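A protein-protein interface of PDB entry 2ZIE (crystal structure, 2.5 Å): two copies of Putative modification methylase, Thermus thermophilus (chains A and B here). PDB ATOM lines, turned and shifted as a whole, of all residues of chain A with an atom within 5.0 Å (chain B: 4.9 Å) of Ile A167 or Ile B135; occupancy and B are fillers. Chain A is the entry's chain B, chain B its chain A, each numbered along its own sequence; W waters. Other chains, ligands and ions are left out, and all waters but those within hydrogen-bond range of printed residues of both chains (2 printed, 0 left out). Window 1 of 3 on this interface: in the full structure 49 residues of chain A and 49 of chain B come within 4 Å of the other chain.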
ATOM      1  N   GLY A  98     -33.473   7.345  -7.669  1.00  0.00           N
ATOM      2  CA  GLY A  98     -32.776   8.600  -7.857  1.00  0.00           C
ATOM      3  C   GLY A  98     -32.790   9.275  -6.498  1.00  0.00           C
ATOM      4  O   GLY A  98     -33.757   9.121  -5.763  1.00  0.00           O
ATOM      5  N   ILE A 135     -24.852   2.558 -12.608  1.00  0.00           N
ATOM      6  CA  ILE A 135     -25.184   3.965 -12.631  1.00  0.00           C
ATOM      7  C   ILE A 135     -25.945   4.256 -13.919  1.00  0.00           C
ATOM      8  O   ILE A 135     -25.449   4.003 -15.009  1.00  0.00           O
ATOM      9  CB  ILE A 135     -23.925   4.861 -12.609  1.00  0.00           C
ATOM     10  CG1 ILE A 135     -23.096   4.583 -11.356  1.00  0.00           C
ATOM     11  CG2 ILE A 135     -24.339   6.334 -12.681  1.00  0.00           C
ATOM     12  CD1 ILE A 135     -23.842   4.761 -10.072  1.00  0.00           C
ATOM     13  N   TRP A 136     -27.157   4.775 -13.790  1.00  0.00           N
ATOM     14  CA  TRP A 136     -27.949   5.125 -14.956  1.00  0.00           C
ATOM     15  C   TRP A 136     -27.745   6.607 -15.247  1.00  0.00           C
ATOM     16  O   TRP A 136     -28.235   7.464 -14.512  1.00  0.00           O
ATOM     17  CB  TRP A 136     -29.435   4.849 -14.710  1.00  0.00           C
ATOM     18  CG  TRP A 136     -30.322   5.304 -15.838  1.00  0.00           C
ATOM     19  CD1 TRP A 136     -29.977   5.415 -17.150  1.00  0.00           C
ATOM     20  CD2 TRP A 136     -31.708   5.661 -15.758  1.00  0.00           C
ATOM     21  NE1 TRP A 136     -31.052   5.815 -17.891  1.00  0.00           N
ATOM     22  CE2 TRP A 136     -32.132   5.974 -17.066  1.00  0.00           C
ATOM     23  CE3 TRP A 136     -32.634   5.746 -14.705  1.00  0.00           C
ATOM     24  CZ2 TRP A 136     -33.448   6.366 -17.362  1.00  0.00           C
ATOM     25  CZ3 TRP A 136     -33.942   6.137 -14.995  1.00  0.00           C
ATOM     26  CH2 TRP A 136     -34.337   6.442 -16.320  1.00  0.00           C
ATOM     27  N   HIS A 137     -27.001   6.907 -16.307  1.00  0.00           N
ATOM     28  CA  HIS A 137     -26.779   8.298 -16.672  1.00  0.00           C
ATOM     29  C   HIS A 137     -28.004   8.762 -17.456  1.00  0.00           C
ATOM     30  O   HIS A 137     -28.024   8.696 -18.674  1.00  0.00           O
ATOM     31  CB  HIS A 137     -25.512   8.435 -17.516  1.00  0.00           C
ATOM     32  CG  HIS A 137     -24.904   9.803 -17.466  1.00  0.00           C
ATOM     33  ND1 HIS A 137     -23.726  10.122 -18.105  1.00  0.00           N
ATOM     34  CD2 HIS A 137     -25.307  10.933 -16.837  1.00  0.00           C
ATOM     35  CE1 HIS A 137     -23.430  11.387 -17.873  1.00  0.00           C
ATOM     36  NE2 HIS A 137     -24.372  11.902 -17.105  1.00  0.00           N
ATOM     37  N   LYS A 138     -29.028   9.188 -16.719  1.00  0.00           N
ATOM     38  CA  LYS A 138     -30.308   9.663 -17.244  1.00  0.00           C
ATOM     39  C   LYS A 138     -30.189  10.867 -18.152  1.00  0.00           C
ATOM     40  O   LYS A 138     -30.609  10.844 -19.306  1.00  0.00           O
ATOM     41  CB  LYS A 138     -31.236  10.071 -16.092  1.00  0.00           C
ATOM     42  CG  LYS A 138     -32.229   9.033 -15.654  1.00  0.00           C
ATOM     43  CD  LYS A 138     -33.665   9.518 -15.824  1.00  0.00           C
ATOM     44  CE  LYS A 138     -34.104  10.461 -14.712  1.00  0.00           C
ATOM     45  NZ  LYS A 138     -35.557  10.821 -14.853  1.00  0.00           N
ATOM     46  N   THR A 165     -28.425  17.162 -10.919  1.00  0.00           N
ATOM     47  CA  THR A 165     -28.581  15.716 -10.997  1.00  0.00           C
ATOM     48  C   THR A 165     -28.625  15.150 -12.410  1.00  0.00           C
ATOM     49  O   THR A 165     -29.414  15.578 -13.236  1.00  0.00           O
ATOM     50  CB  THR A 165     -29.843  15.268 -10.277  1.00  0.00           C
ATOM     51  OG1 THR A 165     -29.753  15.651  -8.907  1.00  0.00           O
ATOM     52  CG2 THR A 165     -29.993  13.781 -10.356  1.00  0.00           C
ATOM     53  N   GLU A 166     -27.792  14.160 -12.674  1.00  0.00           N
ATOM     54  CA  GLU A 166     -27.759  13.549 -13.988  1.00  0.00           C
ATOM     55  C   GLU A 166     -27.960  12.043 -13.898  1.00  0.00           C
ATOM     56  O   GLU A 166     -28.176  11.379 -14.905  1.00  0.00           O
ATOM     57  CB  GLU A 166     -26.409  13.812 -14.645  1.00  0.00           C
ATOM     58  CG  GLU A 166     -26.092  15.264 -14.881  1.00  0.00           C
ATOM     59  CD  GLU A 166     -24.653  15.469 -15.299  1.00  0.00           C
ATOM     60  OE1 GLU A 166     -24.129  14.620 -16.054  1.00  0.00           O
ATOM     61  OE2 GLU A 166     -24.043  16.480 -14.884  1.00  0.00           O
ATOM     62  N   ILE A 167     -27.911  11.507 -12.687  1.00  0.00           N
ATOM     63  CA  ILE A 167     -27.997  10.065 -12.523  1.00  0.00           C
ATOM     64  C   ILE A 167     -29.028   9.482 -11.564  1.00  0.00           C
ATOM     65  O   ILE A 167     -29.663  10.179 -10.781  1.00  0.00           O
ATOM     66  CB  ILE A 167     -26.632   9.518 -12.062  1.00  0.00           C
ATOM     67  CG1 ILE A 167     -26.311  10.064 -10.671  1.00  0.00           C
ATOM     68  CG2 ILE A 167     -25.540   9.934 -13.038  1.00  0.00           C
ATOM     69  CD1 ILE A 167     -25.253   9.322  -9.933  1.00  0.00           C
ATOM     70  N   GLU A 168     -29.161   8.165 -11.650  1.00  0.00           N
ATOM     71  CA  GLU A 168     -30.024   7.388 -10.778  1.00  0.00           C
ATOM     72  C   GLU A 168     -29.242   6.112 -10.527  1.00  0.00           C
ATOM     73  O   GLU A 168     -28.382   5.739 -11.327  1.00  0.00           O
ATOM     74  CB  GLU A 168     -31.376   7.090 -11.429  1.00  0.00           C
ATOM     75  CG  GLU A 168     -32.378   8.210 -11.227  1.00  0.00           C
ATOM     76  CD  GLU A 168     -33.780   7.823 -11.628  1.00  0.00           C
ATOM     77  OE1 GLU A 168     -34.179   6.686 -11.324  1.00  0.00           O
ATOM     78  OE2 GLU A 168     -34.492   8.652 -12.231  1.00  0.00           O
ATOM     79  N   TYR A 169     -29.513   5.458  -9.403  1.00  0.00           N
ATOM     80  CA  TYR A 169     -28.803   4.235  -9.051  1.00  0.00           C
ATOM     81  C   TYR A 169     -29.620   2.987  -9.286  1.00  0.00           C
ATOM     82  O   TYR A 169     -30.806   2.944  -8.977  1.00  0.00           O
ATOM     83  CB  TYR A 169     -28.381   4.282  -7.589  1.00  0.00           C
ATOM     84  CG  TYR A 169     -27.679   5.561  -7.234  1.00  0.00           C
ATOM     85  CD1 TYR A 169     -26.299   5.609  -7.090  1.00  0.00           C
ATOM     86  CD2 TYR A 169     -28.404   6.734  -7.049  1.00  0.00           C
ATOM     87  CE1 TYR A 169     -25.660   6.796  -6.763  1.00  0.00           C
ATOM     88  CE2 TYR A 169     -27.777   7.919  -6.728  1.00  0.00           C
ATOM     89  CZ  TYR A 169     -26.407   7.944  -6.582  1.00  0.00           C
ATOM     90  OH  TYR A 169     -25.804   9.120  -6.220  1.00  0.00           O
ATOM     91  N   ILE A 204     -21.839   1.658 -16.042  1.00  0.00           N
ATOM     92  CA  ILE A 204     -22.594   2.867 -16.361  1.00  0.00           C
ATOM     93  C   ILE A 204     -23.387   2.735 -17.653  1.00  0.00           C
ATOM     94  O   ILE A 204     -22.864   2.268 -18.656  1.00  0.00           O
ATOM     95  CB  ILE A 204     -21.679   4.126 -16.494  1.00  0.00           C
ATOM     96  CG1 ILE A 204     -20.804   4.277 -15.252  1.00  0.00           C
ATOM     97  CG2 ILE A 204     -22.540   5.381 -16.652  1.00  0.00           C
ATOM     98  CD1 ILE A 204     -19.976   5.531 -15.235  1.00  0.00           C
ATOM     99  N   PRO B 133     -23.360  13.319  -5.074  1.00  0.00           N
ATOM    100  CA  PRO B 133     -21.961  12.939  -5.259  1.00  0.00           C
ATOM    101  C   PRO B 133     -21.558  12.963  -6.726  1.00  0.00           C
ATOM    102  O   PRO B 133     -22.400  12.945  -7.612  1.00  0.00           O
ATOM    103  CB  PRO B 133     -21.927  11.538  -4.675  1.00  0.00           C
ATOM    104  CG  PRO B 133     -23.247  10.988  -5.154  1.00  0.00           C
ATOM    105  CD  PRO B 133     -24.214  12.130  -4.905  1.00  0.00           C
ATOM    106  N   ILE B 134     -20.261  13.030  -6.970  1.00  0.00           N
ATOM    107  CA  ILE B 134     -19.749  13.007  -8.318  1.00  0.00           C
ATOM    108  C   ILE B 134     -19.242  11.589  -8.493  1.00  0.00           C
ATOM    109  O   ILE B 134     -18.653  11.007  -7.576  1.00  0.00           O
ATOM    110  CB  ILE B 134     -18.586  13.990  -8.505  1.00  0.00           C
ATOM    111  CG1 ILE B 134     -19.106  15.419  -8.405  1.00  0.00           C
ATOM    112  CG2 ILE B 134     -17.925  13.777  -9.867  1.00  0.00           C
ATOM    113  CD1 ILE B 134     -18.019  16.465  -8.480  1.00  0.00           C
ATOM    114  N   ILE B 135     -19.499  11.024  -9.664  1.00  0.00           N
ATOM    115  CA  ILE B 135     -19.052   9.677  -9.951  1.00  0.00           C
ATOM    116  C   ILE B 135     -17.734   9.742 -10.705  1.00  0.00           C
ATOM    117  O   ILE B 135     -17.646  10.341 -11.775  1.00  0.00           O
ATOM    118  CB  ILE B 135     -20.087   8.890 -10.790  1.00  0.00           C
ATOM    119  CG1 ILE B 135     -21.231   8.394  -9.907  1.00  0.00           C
ATOM    120  CG2 ILE B 135     -19.431   7.646 -11.381  1.00  0.00           C
ATOM    121  CD1 ILE B 135     -21.885   9.426  -9.108  1.00  0.00           C
ATOM    122  N   TRP B 136     -16.703   9.152 -10.124  1.00  0.00           N
ATOM    123  CA  TRP B 136     -15.409   9.123 -10.768  1.00  0.00           C
ATOM    124  C   TRP B 136     -15.290   7.818 -11.540  1.00  0.00           C
ATOM    125  O   TRP B 136     -15.136   6.743 -10.961  1.00  0.00           O
ATOM    126  CB  TRP B 136     -14.279   9.224  -9.740  1.00  0.00           C
ATOM    127  CG  TRP B 136     -12.902   9.074 -10.343  1.00  0.00           C
ATOM    128  CD1 TRP B 136     -12.504   9.478 -11.586  1.00  0.00           C
ATOM    129  CD2 TRP B 136     -11.730   8.571  -9.692  1.00  0.00           C
ATOM    130  NE1 TRP B 136     -11.160   9.267 -11.746  1.00  0.00           N
ATOM    131  CE2 TRP B 136     -10.657   8.712 -10.601  1.00  0.00           C
ATOM    132  CE3 TRP B 136     -11.480   8.019  -8.427  1.00  0.00           C
ATOM    133  CZ2 TRP B 136      -9.345   8.321 -10.285  1.00  0.00           C
ATOM    134  CZ3 TRP B 136     -10.172   7.629  -8.110  1.00  0.00           C
ATOM    135  CH2 TRP B 136      -9.125   7.785  -9.040  1.00  0.00           C
ATOM    136  N   HIS B 137     -15.388   7.910 -12.857  1.00  0.00           N
ATOM    137  CA  HIS B 137     -15.267   6.723 -13.666  1.00  0.00           C
ATOM    138  C   HIS B 137     -13.783   6.478 -13.895  1.00  0.00           C
ATOM    139  O   HIS B 137     -13.220   6.986 -14.850  1.00  0.00           O
ATOM    140  CB  HIS B 137     -15.982   6.915 -14.991  1.00  0.00           C
ATOM    141  CG  HIS B 137     -16.272   5.634 -15.694  1.00  0.00           C
ATOM    142  ND1 HIS B 137     -16.979   5.574 -16.873  1.00  0.00           N
ATOM    143  CD2 HIS B 137     -15.950   4.356 -15.382  1.00  0.00           C
ATOM    144  CE1 HIS B 137     -17.081   4.316 -17.257  1.00  0.00           C
ATOM    145  NE2 HIS B 137     -16.464   3.558 -16.370  1.00  0.00           N
ATOM    146  N   ILE B 167     -16.007   2.373 -10.934  1.00  0.00           N
ATOM    147  CA  ILE B 167     -16.147   3.683 -10.332  1.00  0.00           C
ATOM    148  C   ILE B 167     -15.807   3.820  -8.868  1.00  0.00           C
ATOM    149  O   ILE B 167     -15.717   2.849  -8.127  1.00  0.00           O
ATOM    150  CB  ILE B 167     -17.604   4.172 -10.460  1.00  0.00           C
ATOM    151  CG1 ILE B 167     -18.478   3.386  -9.471  1.00  0.00           C
ATOM    152  CG2 ILE B 167     -18.096   3.993 -11.898  1.00  0.00           C
ATOM    153  CD1 ILE B 167     -19.896   3.827  -9.381  1.00  0.00           C
ATOM    154  N   GLU B 168     -15.652   5.072  -8.470  1.00  0.00           N
ATOM    155  CA  GLU B 168     -15.413   5.435  -7.089  1.00  0.00           C
ATOM    156  C   GLU B 168     -16.378   6.583  -6.872  1.00  0.00           C
ATOM    157  O   GLU B 168     -16.736   7.274  -7.819  1.00  0.00           O
ATOM    158  CB  GLU B 168     -13.974   5.877  -6.868  1.00  0.00           C
ATOM    159  CG  GLU B 168     -13.055   4.723  -6.555  1.00  0.00           C
ATOM    160  CD  GLU B 168     -11.765   5.179  -5.927  1.00  0.00           C
ATOM    161  OE1 GLU B 168     -11.824   6.057  -5.048  1.00  0.00           O
ATOM    162  OE2 GLU B 168     -10.696   4.659  -6.297  1.00  0.00           O
ATOM    163  N   GLN B 203     -21.876  15.653 -13.066  1.00  0.00           N
ATOM    164  CA  GLN B 203     -21.935  14.535 -12.152  1.00  0.00           C
ATOM    165  C   GLN B 203     -20.995  13.339 -12.418  1.00  0.00           C
ATOM    166  O   GLN B 203     -20.675  12.604 -11.489  1.00  0.00           O
ATOM    167  CB  GLN B 203     -23.387  14.087 -11.997  1.00  0.00           C
ATOM    168  CG  GLN B 203     -23.571  13.125 -10.851  1.00  0.00           C
ATOM    169  CD  GLN B 203     -24.974  13.127 -10.286  1.00  0.00           C
ATOM    170  OE1 GLN B 203     -25.938  13.342 -11.010  1.00  0.00           O
ATOM    171  NE2 GLN B 203     -25.095  12.865  -8.984  1.00  0.00           N
ATOM    172  N   ILE B 204     -20.539  13.140 -13.652  1.00  0.00           N
ATOM    173  CA  ILE B 204     -19.620  12.027 -13.933  1.00  0.00           C
ATOM    174  C   ILE B 204     -18.286  12.541 -14.478  1.00  0.00           C
ATOM    175  O   ILE B 204     -18.262  13.294 -15.443  1.00  0.00           O
ATOM    176  CB  ILE B 204     -20.140  11.044 -15.031  1.00  0.00           C
ATOM    177  CG1 ILE B 204     -21.601  10.671 -14.820  1.00  0.00           C
ATOM    178  CG2 ILE B 204     -19.283   9.791 -15.031  1.00  0.00           C
ATOM    179  CD1 ILE B 204     -21.833   9.776 -13.673  1.00  0.00           C
ATOM    180  N   TRP B 205     -17.178  12.139 -13.862  1.00  0.00           N
ATOM    181  CA  TRP B 205     -15.867  12.520 -14.359  1.00  0.00           C
ATOM    182  C   TRP B 205     -15.255  11.283 -14.993  1.00  0.00           C
ATOM    183  O   TRP B 205     -15.040  10.277 -14.315  1.00  0.00           O
ATOM    184  CB  TRP B 205     -14.948  12.983 -13.244  1.00  0.00           C
ATOM    185  CG  TRP B 205     -15.231  14.344 -12.735  1.00  0.00           C
ATOM    186  CD1 TRP B 205     -16.122  15.242 -13.238  1.00  0.00           C
ATOM    187  CD2 TRP B 205     -14.655  14.953 -11.576  1.00  0.00           C
ATOM    188  NE1 TRP B 205     -16.146  16.371 -12.459  1.00  0.00           N
ATOM    189  CE2 TRP B 205     -15.255  16.221 -11.432  1.00  0.00           C
ATOM    190  CE3 TRP B 205     -13.690  14.546 -10.643  1.00  0.00           C
ATOM    191  CZ2 TRP B 205     -14.926  17.093 -10.388  1.00  0.00           C
ATOM    192  CZ3 TRP B 205     -13.361  15.408  -9.607  1.00  0.00           C
ATOM    193  CH2 TRP B 205     -13.980  16.671  -9.488  1.00  0.00           C
HETATM  194  O   HOH W   1     -21.492  14.181 -16.795  1.00  0.00           O
HETATM  195  O   HOH W   2     -27.298  11.257  -6.883  1.00  0.00           O
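The backbone NH (N) of Glu A166 sits at hydrogen-bond distance from the side-chain amide oxygen (OE1) of Gln B203 (2.6 Å). OE1 of Gln B203 lies within hydrogen-bond range of N of Ile A167 (3.2 Å).
O of Pro B133 lies within hydrogen-bond range of NE2 of Gln B203 (3.0 Å). N of Ile B135 sits at hydrogen-bond distance from O of Gln B203 (2.7 Å). The backbone carbonyl oxygen (O) of Ile B135 lies within hydrogen-bond range of the backbone NH (N) of Trp B205, 2.8 Å away. The backbone NH (N) of His B137 lies within hydrogen-bond range of the backbone carbonyl oxygen (O) of Trp B205 (2.8 Å). The side-chain carboxylate (OE1) of Glu A166 lies within hydrogen-bond range of a ring nitrogen (NE2) of His A137. The backbone NH (N) of Lys A138 is in hydrogen-bond range of the backbone carbonyl oxygen (O) of Glu A166, at 3.0 Å.
Ile B167 touches Ile A135 (CD1 to CG1, 3.8 Å). Ile B204 touches His A137. Thr A165 touches Gln B203. Ile B135 touches Ile A167 (CD1 to CD1, 3.5 Å). Ile B204 touches Ile A167. CG of Pro B133 touches OH of Tyr A169 (3.3 Å). ND1 of His B137 touches CD1 of Ile A204 (3.4 Å).
Of chain B, only Ile B135 (3.5 Å), Gln B203 (3.2 Å) and Ile B204 (3.8 Å) come within 4 Å of Ile A167. Of chain A, only Ile A167 comes within 4 Å of Ile B135. Of the printed residues of chain B, Tyr A169 touches Pro B133 (3.3 Å). Printed residues of chain B within 4 Å of Glu A166: Gln B203. Printed residues of chain A within 4 Å of Gln B203: Thr A165, Glu A166 and Ile A167. The nearest printed residue of chain B that does not touch Ile A167 is Pro B133 (5.2 Å). The nearest residue of chain A that does not touch Ile B135 is Ile A204 (4.4 Å). The nearest printed residue of chain A that does not touch Ile B204 is Ile A204 (4.3 Å).
Hydrophobic or aromatic side chains of chain A that line the printed part of chain B: Ile A135, His A137, Ile A167, Tyr A169 and Ile A204. Of the 10 printed residues of chain B, 6 touch a printed residue of chain A. Printed residues of chain B that touch a printed residue of chain A: Pro B133, Ile B135, His B137, Ile B167, Gln B203 and Ile B204. Hydrophobic or aromatic side chains of chain B within 4 Å of the printed part of chain A: Pro B133, Ile B135, His B137, Ile B167 and Ile B204. Among the printed residues, 9 pairs touch across the chains.
Ile A135 touches Ile B167, and with the chains exchanged Ile A167 touches Ile B135. His A137 touches Ile B204, and with the chains exchanged Ile A204 touches His B137. Ile A167 touches Ile B204, but with the chains exchanged Ile A204 does not touch Ile B167 (4.1 Å). Of the 9 pairs that touch across the chains among the printed residues, 4 have their exchanged pair printed and touching as well.
Water W2 lies within hydrogen-bond range of OH of Tyr A169 (2.7 Å) and NE2 of Gln B203 (3.4 Å). Water W1 lies within hydrogen-bond range of OE1 of Glu A166 (2.8 Å) and N of Ile B204 (3.4 Å).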
